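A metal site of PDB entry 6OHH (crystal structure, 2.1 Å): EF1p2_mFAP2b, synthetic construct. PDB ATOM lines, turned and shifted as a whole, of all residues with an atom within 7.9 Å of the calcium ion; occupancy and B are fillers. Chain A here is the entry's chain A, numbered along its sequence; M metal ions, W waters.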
ATOM      1  N   GLY A  79     -20.027  19.587  12.229  1.00  0.00           N
ATOM      2  CA  GLY A  79     -19.792  20.976  11.847  1.00  0.00           C
ATOM      3  C   GLY A  79     -18.975  21.778  12.831  1.00  0.00           C
ATOM      4  O   GLY A  79     -19.197  22.988  12.990  1.00  0.00           O
ATOM      5  N   GLY A 103     -22.938  25.770  17.879  1.00  0.00           N
ATOM      6  CA  GLY A 103     -22.227  25.800  16.623  1.00  0.00           C
ATOM      7  C   GLY A 103     -23.022  25.163  15.509  1.00  0.00           C
ATOM      8  O   GLY A 103     -24.145  24.695  15.699  1.00  0.00           O
ATOM      9  N   ASP A 104     -22.406  25.119  14.327  1.00  0.00           N
ATOM     10  CA  ASP A 104     -23.028  24.632  13.107  1.00  0.00           C
ATOM     11  C   ASP A 104     -23.185  23.116  13.099  1.00  0.00           C
ATOM     12  O   ASP A 104     -22.526  22.417  12.321  1.00  0.00           O
ATOM     13  CB  ASP A 104     -22.206  25.092  11.894  1.00  0.00           C
ATOM     14  CG  ASP A 104     -22.847  24.746  10.562  1.00  0.00           C
ATOM     15  OD1 ASP A 104     -24.093  24.630  10.508  1.00  0.00           O
ATOM     16  OD2 ASP A 104     -22.115  24.578   9.567  1.00  0.00           O
ATOM     17  N   LYS A 105     -24.073  22.609  13.955  1.00  0.00           N
ATOM     18  CA  LYS A 105     -24.218  21.154  14.110  1.00  0.00           C
ATOM     19  C   LYS A 105     -24.594  20.460  12.805  1.00  0.00           C
ATOM     20  O   LYS A 105     -24.094  19.369  12.526  1.00  0.00           O
ATOM     21  CB  LYS A 105     -25.235  20.844  15.211  1.00  0.00           C
ATOM     22  CG  LYS A 105     -25.084  19.440  15.753  1.00  0.00           C
ATOM     23  CD  LYS A 105     -26.071  19.146  16.876  1.00  0.00           C
ATOM     24  CE  LYS A 105     -25.694  17.856  17.596  1.00  0.00           C
ATOM     25  NZ  LYS A 105     -26.541  17.602  18.792  1.00  0.00           N
ATOM     26  N   ASP A 106     -25.493  21.047  12.009  1.00  0.00           N
ATOM     27  CA  ASP A 106     -25.892  20.384  10.770  1.00  0.00           C
ATOM     28  C   ASP A 106     -24.908  20.582   9.628  1.00  0.00           C
ATOM     29  O   ASP A 106     -25.132  20.038   8.541  1.00  0.00           O
ATOM     30  CB  ASP A 106     -27.295  20.827  10.334  1.00  0.00           C
ATOM     31  CG  ASP A 106     -27.382  22.311   9.981  1.00  0.00           C
ATOM     32  OD1 ASP A 106     -26.344  22.961   9.743  1.00  0.00           O
ATOM     33  OD2 ASP A 106     -28.518  22.821   9.923  1.00  0.00           O
ATOM     34  N   GLY A 107     -23.844  21.356   9.842  1.00  0.00           N
ATOM     35  CA  GLY A 107     -22.779  21.507   8.861  1.00  0.00           C
ATOM     36  C   GLY A 107     -23.165  22.164   7.559  1.00  0.00           C
ATOM     37  O   GLY A 107     -22.477  21.973   6.549  1.00  0.00           O
ATOM     38  N   ASP A 108     -24.229  22.963   7.532  1.00  0.00           N
ATOM     39  CA  ASP A 108     -24.644  23.639   6.314  1.00  0.00           C
ATOM     40  C   ASP A 108     -23.945  24.982   6.114  1.00  0.00           C
ATOM     41  O   ASP A 108     -24.204  25.659   5.105  1.00  0.00           O
ATOM     42  CB  ASP A 108     -26.167  23.822   6.285  1.00  0.00           C
ATOM     43  CG  ASP A 108     -26.662  24.856   7.285  1.00  0.00           C
ATOM     44  OD1 ASP A 108     -25.861  25.360   8.113  1.00  0.00           O
ATOM     45  OD2 ASP A 108     -27.870  25.171   7.262  1.00  0.00           O
ATOM     46  N   GLY A 109     -23.055  25.376   7.026  1.00  0.00           N
ATOM     47  CA  GLY A 109     -22.309  26.601   6.919  1.00  0.00           C
ATOM     48  C   GLY A 109     -22.954  27.826   7.528  1.00  0.00           C
ATOM     49  O   GLY A 109     -22.299  28.877   7.597  1.00  0.00           O
ATOM     50  N   TYR A 110     -24.202  27.735   7.978  1.00  0.00           N
ATOM     51  CA  TYR A 110     -24.928  28.860   8.568  1.00  0.00           C
ATOM     52  C   TYR A 110     -25.402  28.491   9.973  1.00  0.00           C
ATOM     53  O   TYR A 110     -25.818  27.359  10.223  1.00  0.00           O
ATOM     54  CB  TYR A 110     -26.119  29.267   7.695  1.00  0.00           C
ATOM     55  N   ILE A 111     -25.345  29.454  10.884  1.00  0.00           N
ATOM     56  CA  ILE A 111     -25.761  29.240  12.266  1.00  0.00           C
ATOM     57  C   ILE A 111     -27.234  29.602  12.394  1.00  0.00           C
ATOM     58  O   ILE A 111     -27.612  30.771  12.337  1.00  0.00           O
ATOM     59  CB  ILE A 111     -24.894  30.063  13.241  1.00  0.00           C
ATOM     60  CG1 ILE A 111     -23.415  29.721  13.090  1.00  0.00           C
ATOM     61  CG2 ILE A 111     -25.356  29.836  14.678  1.00  0.00           C
ATOM     62  CD1 ILE A 111     -23.023  28.389  13.710  1.00  0.00           C
ATOM     63  N   SER A 112     -28.079  28.587  12.548  1.00  0.00           N
ATOM     64  CA  SER A 112     -29.510  28.759  12.733  1.00  0.00           C
ATOM     65  C   SER A 112     -29.810  29.096  14.196  1.00  0.00           C
ATOM     66  O   SER A 112     -28.917  29.116  15.052  1.00  0.00           O
ATOM     67  CB  SER A 112     -30.257  27.510  12.284  1.00  0.00           C
ATOM     68  OG  SER A 112     -29.967  26.415  13.136  1.00  0.00           O
ATOM     69  N   ALA A 113     -31.082  29.364  14.500  1.00  0.00           N
ATOM     70  CA  ALA A 113     -31.460  29.697  15.869  1.00  0.00           C
ATOM     71  C   ALA A 113     -31.148  28.558  16.835  1.00  0.00           C
ATOM     72  O   ALA A 113     -30.584  28.780  17.914  1.00  0.00           O
ATOM     73  CB  ALA A 113     -32.945  30.048  15.929  1.00  0.00           C
ATOM     74  N   GLU A 115     -28.855  26.461  16.641  1.00  0.00           N
ATOM     75  CA  GLU A 115     -27.404  26.389  16.729  1.00  0.00           C
ATOM     76  C   GLU A 115     -26.780  27.585  17.462  1.00  0.00           C
ATOM     77  O   GLU A 115     -25.603  27.500  17.829  1.00  0.00           O
ATOM     78  CB  GLU A 115     -26.833  26.278  15.323  1.00  0.00           C
ATOM     79  CG  GLU A 115     -27.114  24.925  14.684  1.00  0.00           C
ATOM     80  CD  GLU A 115     -26.808  24.915  13.205  1.00  0.00           C
ATOM     81  OE1 GLU A 115     -26.584  26.001  12.643  1.00  0.00           O
ATOM     82  OE2 GLU A 115     -26.790  23.813  12.605  1.00  0.00           O
HETATM   83 CA    CA M   1     -26.294  25.138  10.416  1.00  0.00          CA
HETATM   84  O   HOH W   1     -28.622  25.364  10.088  1.00  0.00           O
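The side-chain carboxylate of Glu 115 sits close to the backbone NH of Lys 105 (3.3 Å). OD1 of Asp 104 lies close to N of Gly 107, at 3.4 Å. OE1 of Glu 115 sits close to N of Ser 112 (3.0 Å). The backbone NH of Gly 103 sits at hydrogen-bond distance from the backbone carbonyl oxygen of Glu 115 (3.2 Å). The side-chain carboxylate (OD2) of Asp 104 lies within hydrogen-bond range of the backbone NH (N) of Gly 109, 2.8 Å away.
The calcium ion is bound by OD1 of Asp 104 (2.3 Å), O of Tyr 110 (2.3 Å), OD1 of Asp 106 (2.3 Å), OD1 of Asp 108 (2.4 Å), water W1 (2.4 Å), OE1 of Glu 115 (2.4 Å) and OE2 of Glu 115 (2.6 Å).
Water W1 lies within hydrogen-bond range of the side-chain carboxylate (OD2) of Asp 106 (2.6 Å), the side-chain carboxylate (OD2) of Asp 108 (2.9 Å) and the side-chain hydroxyl (OG) of Ser 112 (3.5 Å).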
